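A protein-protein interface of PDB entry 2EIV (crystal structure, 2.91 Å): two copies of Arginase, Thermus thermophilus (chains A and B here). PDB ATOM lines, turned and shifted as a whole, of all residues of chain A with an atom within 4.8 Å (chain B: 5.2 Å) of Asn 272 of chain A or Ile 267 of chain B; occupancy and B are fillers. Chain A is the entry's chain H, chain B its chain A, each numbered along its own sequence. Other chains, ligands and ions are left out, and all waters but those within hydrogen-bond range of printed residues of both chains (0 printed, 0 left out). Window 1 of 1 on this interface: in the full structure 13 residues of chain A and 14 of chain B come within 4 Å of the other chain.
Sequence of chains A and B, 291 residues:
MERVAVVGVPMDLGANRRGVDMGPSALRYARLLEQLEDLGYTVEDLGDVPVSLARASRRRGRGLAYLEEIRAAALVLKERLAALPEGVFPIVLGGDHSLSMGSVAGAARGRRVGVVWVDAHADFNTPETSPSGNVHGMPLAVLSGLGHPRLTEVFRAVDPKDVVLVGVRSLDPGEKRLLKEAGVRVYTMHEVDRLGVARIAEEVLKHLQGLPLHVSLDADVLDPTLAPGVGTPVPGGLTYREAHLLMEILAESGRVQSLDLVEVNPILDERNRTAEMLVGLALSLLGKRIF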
ATOM      1  N   ALA A  26      -7.330  13.034 -30.758  1.00  0.00           N
ATOM      2  CA  ALA A  26      -6.441  11.896 -30.589  1.00  0.00           C
ATOM      3  C   ALA A  26      -4.993  12.333 -30.745  1.00  0.00           C
ATOM      4  O   ALA A  26      -4.090  11.795 -30.108  1.00  0.00           O
ATOM      5  CB  ALA A  26      -6.770  10.839 -31.600  1.00  0.00           C
ATOM      6  N   TYR A  29      -4.016  13.657 -27.435  1.00  0.00           N
ATOM      7  CA  TYR A  29      -3.833  12.608 -26.440  1.00  0.00           C
ATOM      8  C   TYR A  29      -2.583  11.776 -26.697  1.00  0.00           C
ATOM      9  O   TYR A  29      -2.140  11.017 -25.832  1.00  0.00           O
ATOM     10  CB  TYR A  29      -5.079  11.728 -26.378  1.00  0.00           C
ATOM     11  CG  TYR A  29      -6.170  12.386 -25.563  1.00  0.00           C
ATOM     12  CD1 TYR A  29      -6.393  12.017 -24.234  1.00  0.00           C
ATOM     13  CD2 TYR A  29      -6.940  13.427 -26.095  1.00  0.00           C
ATOM     14  CE1 TYR A  29      -7.359  12.673 -23.451  1.00  0.00           C
ATOM     15  CE2 TYR A  29      -7.903  14.091 -25.324  1.00  0.00           C
ATOM     16  CZ  TYR A  29      -8.106  13.709 -24.003  1.00  0.00           C
ATOM     17  OH  TYR A  29      -9.039  14.365 -23.234  1.00  0.00           O
ATOM     18  N   ALA A  30      -2.015  11.939 -27.889  1.00  0.00           N
ATOM     19  CA  ALA A  30      -0.799  11.246 -28.275  1.00  0.00           C
ATOM     20  C   ALA A  30       0.388  12.122 -27.896  1.00  0.00           C
ATOM     21  O   ALA A  30       1.515  11.926 -28.354  1.00  0.00           O
ATOM     22  CB  ALA A  30      -0.801  11.005 -29.753  1.00  0.00           C
ATOM     23  N   ASP A 269      -9.501   3.372 -35.425  1.00  0.00           N
ATOM     24  CA  ASP A 269      -8.147   3.061 -34.960  1.00  0.00           C
ATOM     25  C   ASP A 269      -8.087   1.988 -33.886  1.00  0.00           C
ATOM     26  O   ASP A 269      -9.106   1.482 -33.424  1.00  0.00           O
ATOM     27  CB  ASP A 269      -7.489   4.337 -34.447  1.00  0.00           C
ATOM     28  CG  ASP A 269      -5.978   4.346 -34.661  1.00  0.00           C
ATOM     29  OD1 ASP A 269      -5.469   3.348 -35.207  1.00  0.00           O
ATOM     30  OD2 ASP A 269      -5.295   5.341 -34.290  1.00  0.00           O
ATOM     31  N   GLU A 270      -6.881   1.611 -33.511  1.00  0.00           N
ATOM     32  CA  GLU A 270      -6.703   0.630 -32.457  1.00  0.00           C
ATOM     33  C   GLU A 270      -5.661   1.207 -31.511  1.00  0.00           C
ATOM     34  O   GLU A 270      -4.619   1.697 -31.952  1.00  0.00           O
ATOM     35  CB  GLU A 270      -6.198  -0.684 -33.029  1.00  0.00           C
ATOM     36  CG  GLU A 270      -6.983  -1.215 -34.211  1.00  0.00           C
ATOM     37  CD  GLU A 270      -6.208  -2.289 -34.933  1.00  0.00           C
ATOM     38  OE1 GLU A 270      -4.992  -2.387 -34.670  1.00  0.00           O
ATOM     39  OE2 GLU A 270      -6.792  -3.021 -35.761  1.00  0.00           O
ATOM     40  N   ARG A 271      -5.944   1.171 -30.215  1.00  0.00           N
ATOM     41  CA  ARG A 271      -5.012   1.699 -29.226  1.00  0.00           C
ATOM     42  C   ARG A 271      -4.553   3.115 -29.623  1.00  0.00           C
ATOM     43  O   ARG A 271      -3.491   3.570 -29.203  1.00  0.00           O
ATOM     44  CB  ARG A 271      -3.794   0.765 -29.098  1.00  0.00           C
ATOM     45  CG  ARG A 271      -4.129  -0.706 -28.771  1.00  0.00           C
ATOM     46  CD  ARG A 271      -4.598  -0.840 -27.339  1.00  0.00           C
ATOM     47  NE  ARG A 271      -5.410  -2.039 -27.134  1.00  0.00           N
ATOM     48  CZ  ARG A 271      -5.822  -2.456 -25.936  1.00  0.00           C
ATOM     49  NH1 ARG A 271      -5.491  -1.770 -24.839  1.00  0.00           N
ATOM     50  NH2 ARG A 271      -6.568  -3.551 -25.830  1.00  0.00           N
ATOM     51  N   ASN A 272      -5.355   3.807 -30.434  1.00  0.00           N
ATOM     52  CA  ASN A 272      -5.039   5.174 -30.868  1.00  0.00           C
ATOM     53  C   ASN A 272      -3.666   5.229 -31.515  1.00  0.00           C
ATOM     54  O   ASN A 272      -2.975   6.233 -31.424  1.00  0.00           O
ATOM     55  CB  ASN A 272      -5.082   6.157 -29.666  1.00  0.00           C
ATOM     56  CG  ASN A 272      -4.999   7.647 -30.095  1.00  0.00           C
ATOM     57  OD1 ASN A 272      -5.711   8.076 -30.993  1.00  0.00           O
ATOM     58  ND2 ASN A 272      -4.131   8.422 -29.442  1.00  0.00           N
ATOM     59  N   ARG A 273      -3.272   4.165 -32.198  1.00  0.00           N
ATOM     60  CA  ARG A 273      -1.944   4.158 -32.778  1.00  0.00           C
ATOM     61  C   ARG A 273      -1.748   4.889 -34.082  1.00  0.00           C
ATOM     62  O   ARG A 273      -0.649   5.352 -34.383  1.00  0.00           O
ATOM     63  CB  ARG A 273      -1.434   2.738 -32.907  1.00  0.00           C
ATOM     64  CG  ARG A 273      -2.288   1.866 -33.759  1.00  0.00           C
ATOM     65  CD  ARG A 273      -1.691   0.480 -33.888  1.00  0.00           C
ATOM     66  NE  ARG A 273      -2.205  -0.108 -35.100  1.00  0.00           N
ATOM     67  CZ  ARG A 273      -2.081  -1.377 -35.429  1.00  0.00           C
ATOM     68  NH1 ARG A 273      -1.442  -2.206 -34.615  1.00  0.00           N
ATOM     69  NH2 ARG A 273      -2.609  -1.811 -36.570  1.00  0.00           N
ATOM     70  N   THR A 274      -2.793   5.001 -34.873  1.00  0.00           N
ATOM     71  CA  THR A 274      -2.625   5.731 -36.099  1.00  0.00           C
ATOM     72  C   THR A 274      -2.228   7.149 -35.688  1.00  0.00           C
ATOM     73  O   THR A 274      -1.334   7.758 -36.278  1.00  0.00           O
ATOM     74  CB  THR A 274      -3.924   5.783 -36.897  1.00  0.00           C
ATOM     75  OG1 THR A 274      -4.386   4.446 -37.156  1.00  0.00           O
ATOM     76  CG2 THR A 274      -3.693   6.556 -38.208  1.00  0.00           C
ATOM     77  N   ALA A 275      -2.884   7.658 -34.650  1.00  0.00           N
ATOM     78  CA  ALA A 275      -2.608   9.010 -34.161  1.00  0.00           C
ATOM     79  C   ALA A 275      -1.178   9.153 -33.632  1.00  0.00           C
ATOM     80  O   ALA A 275      -0.508  10.185 -33.845  1.00  0.00           O
ATOM     81  CB  ALA A 275      -3.605   9.388 -33.075  1.00  0.00           C
ATOM     82  N   GLU A 276      -0.712   8.122 -32.939  1.00  0.00           N
ATOM     83  CA  GLU A 276       0.636   8.161 -32.416  1.00  0.00           C
ATOM     84  C   GLU A 276       1.624   8.215 -33.566  1.00  0.00           C
ATOM     85  O   GLU A 276       2.602   8.961 -33.496  1.00  0.00           O
ATOM     86  CB  GLU A 276       0.913   6.957 -31.531  1.00  0.00           C
ATOM     87  CG  GLU A 276       0.079   6.951 -30.281  1.00  0.00           C
ATOM     88  CD  GLU A 276       0.125   5.615 -29.576  1.00  0.00           C
ATOM     89  OE1 GLU A 276       0.389   4.603 -30.268  1.00  0.00           O
ATOM     90  OE2 GLU A 276      -0.105   5.567 -28.342  1.00  0.00           O
ATOM     91  N   GLY B  19      -8.409   9.298 -22.016  1.00  0.00           N
ATOM     92  CA  GLY B  19      -9.234  10.272 -22.723  1.00  0.00           C
ATOM     93  C   GLY B  19     -10.707   9.893 -22.863  1.00  0.00           C
ATOM     94  O   GLY B  19     -11.209   9.661 -23.965  1.00  0.00           O
ATOM     95  N   MET B  22     -13.717  11.823 -24.911  1.00  0.00           N
ATOM     96  CA  MET B  22     -14.056  11.532 -26.287  1.00  0.00           C
ATOM     97  C   MET B  22     -15.159  10.487 -26.355  1.00  0.00           C
ATOM     98  O   MET B  22     -15.661  10.191 -27.422  1.00  0.00           O
ATOM     99  CB  MET B  22     -12.824  11.017 -27.020  1.00  0.00           C
ATOM    100  CG  MET B  22     -11.686  12.012 -27.140  1.00  0.00           C
ATOM    101  SD  MET B  22     -10.250  11.282 -28.007  1.00  0.00           S
ATOM    102  CE  MET B  22     -10.638  11.536 -29.741  1.00  0.00           C
ATOM    103  N   ASN B 265     -13.590   4.878 -23.223  1.00  0.00           N
ATOM    104  CA  ASN B 265     -12.403   5.553 -23.728  1.00  0.00           C
ATOM    105  C   ASN B 265     -12.037   5.043 -25.112  1.00  0.00           C
ATOM    106  O   ASN B 265     -11.520   3.936 -25.244  1.00  0.00           O
ATOM    107  CB  ASN B 265     -11.210   5.311 -22.787  1.00  0.00           C
ATOM    108  CG  ASN B 265     -10.050   6.260 -23.057  1.00  0.00           C
ATOM    109  OD1 ASN B 265      -9.835   6.686 -24.191  1.00  0.00           O
ATOM    110  ND2 ASN B 265      -9.294   6.586 -22.014  1.00  0.00           N
ATOM    111  N   PRO B 266     -12.310   5.828 -26.167  1.00  0.00           N
ATOM    112  CA  PRO B 266     -11.975   5.397 -27.528  1.00  0.00           C
ATOM    113  C   PRO B 266     -10.465   5.276 -27.791  1.00  0.00           C
ATOM    114  O   PRO B 266     -10.026   4.437 -28.578  1.00  0.00           O
ATOM    115  CB  PRO B 266     -12.630   6.468 -28.393  1.00  0.00           C
ATOM    116  CG  PRO B 266     -12.593   7.667 -27.497  1.00  0.00           C
ATOM    117  CD  PRO B 266     -13.064   7.086 -26.202  1.00  0.00           C
ATOM    118  N   ILE B 267      -9.673   6.108 -27.121  1.00  0.00           N
ATOM    119  CA  ILE B 267      -8.216   6.120 -27.272  1.00  0.00           C
ATOM    120  C   ILE B 267      -7.538   4.807 -26.928  1.00  0.00           C
ATOM    121  O   ILE B 267      -6.411   4.556 -27.352  1.00  0.00           O
ATOM    122  CB  ILE B 267      -7.601   7.219 -26.386  1.00  0.00           C
ATOM    123  CG1 ILE B 267      -7.919   8.595 -26.959  1.00  0.00           C
ATOM    124  CG2 ILE B 267      -6.114   7.056 -26.278  1.00  0.00           C
ATOM    125  CD1 ILE B 267      -8.093   9.629 -25.876  1.00  0.00           C
ATOM    126  N   LEU B 268      -8.227   3.988 -26.141  1.00  0.00           N
ATOM    127  CA  LEU B 268      -7.726   2.689 -25.703  1.00  0.00           C
ATOM    128  C   LEU B 268      -8.526   1.571 -26.310  1.00  0.00           C
ATOM    129  O   LEU B 268      -8.188   0.414 -26.130  1.00  0.00           O
ATOM    130  CB  LEU B 268      -7.816   2.567 -24.179  1.00  0.00           C
ATOM    131  CG  LEU B 268      -6.770   3.336 -23.380  1.00  0.00           C
ATOM    132  CD1 LEU B 268      -7.293   3.637 -22.013  1.00  0.00           C
ATOM    133  CD2 LEU B 268      -5.479   2.539 -23.318  1.00  0.00           C
ATOM    134  N   ASP B 269      -9.577   1.916 -27.037  1.00  0.00           N
ATOM    135  CA  ASP B 269     -10.439   0.906 -27.628  1.00  0.00           C
ATOM    136  C   ASP B 269      -9.908   0.338 -28.945  1.00  0.00           C
ATOM    137  O   ASP B 269      -8.776   0.580 -29.334  1.00  0.00           O
ATOM    138  CB  ASP B 269     -11.856   1.493 -27.794  1.00  0.00           C
ATOM    139  CG  ASP B 269     -12.941   0.428 -27.957  1.00  0.00           C
ATOM    140  OD1 ASP B 269     -12.743  -0.735 -27.533  1.00  0.00           O
ATOM    141  OD2 ASP B 269     -14.014   0.775 -28.501  1.00  0.00           O
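Of the 11 printed residues of chain A, 5 touch a printed residue of chain B. Printed residues of chain A that touch a printed residue of chain B: Ala 26, Tyr 29, Glu 270, Arg 271 and Asn 272. Among the printed residues, 8 pairs touch across the chains. Among the printed residues, no Asp or Glu carboxylate lies within 4 Å of a Lys or Arg side-chain nitrogen of the other chain.
Ala 26 of chain A touches Met 22 of chain B. CE1 of Tyr 29 of chain A touches CA of Gly 19 of chain B (3.1 Å). Tyr 29 of chain A touches Ile 267 of chain B (CD1 to CD1, 3.4 Å). Asp 269 of chain B touches Glu 270 of chain A (O to CA, 3.7 Å). Ile 267 of chain B touches Arg 271 of chain A (O to C, 3.3 Å). Arg 271 of chain A touches Leu 268 of chain B.
The backbone NH (N) of Arg 271 of chain A is in hydrogen-bond range of the backbone carbonyl oxygen (O) of Asp 269 of chain B. O of Ile 267 of chain B sits close to N of Asn 272 of chain A (3.3 Å).
Asn 272 of chain A touches just one residue of chain B: Ile 267. Of chain A, only Tyr 29 (3.4 Å), Arg 271 (3.3 Å) and Asn 272 (3.1 Å) come within 4 Å of Ile 267 of chain B. Printed residues of chain B within 4 Å of Ala 26 of chain A: Met 22 (3.8 Å). Printed residues of chain A within 4 Å of Gly 19 of chain B: Tyr 29. Of the printed residues of chain A, Met 22 of chain B touches Ala 26. Printed residues of chain A within 4 Å of Leu 268 of chain B: Arg 271. Printed residues of chain B within 4 Å of Glu 270 of chain A: Asp 269 (3.7 Å). Asn 265 of chain B touches none of the printed residues of chain A. Ala 275 of chain A touches none of the printed residues of chain B. The nearest printed residue of chain A that does not touch Gly 19 of chain B is Ala 26 of chain A (8.5 Å).
The side-chain amide nitrogen of Asn 272 of chain A sits at hydrogen-bond distance from the backbone carbonyl oxygen of Ala 26 of chain A (3.4 Å). OE1 of Glu 270 of chain A lies within salt-bridge range of NH2 of Arg 273 of chain A (3.1 Å). The backbone NH of Gly 19 of chain B sits close to the side-chain amide nitrogen of Asn 265 of chain B, 2.9 Å away. OD1 of Asn 265 of chain B lies within hydrogen-bond range of N of Ile 267 of chain B (3.0 Å).
1 position is printed for both chains. Of the 8 pairs that touch across the chains among the printed residues, none has its exchanged pair printed and touching as well.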
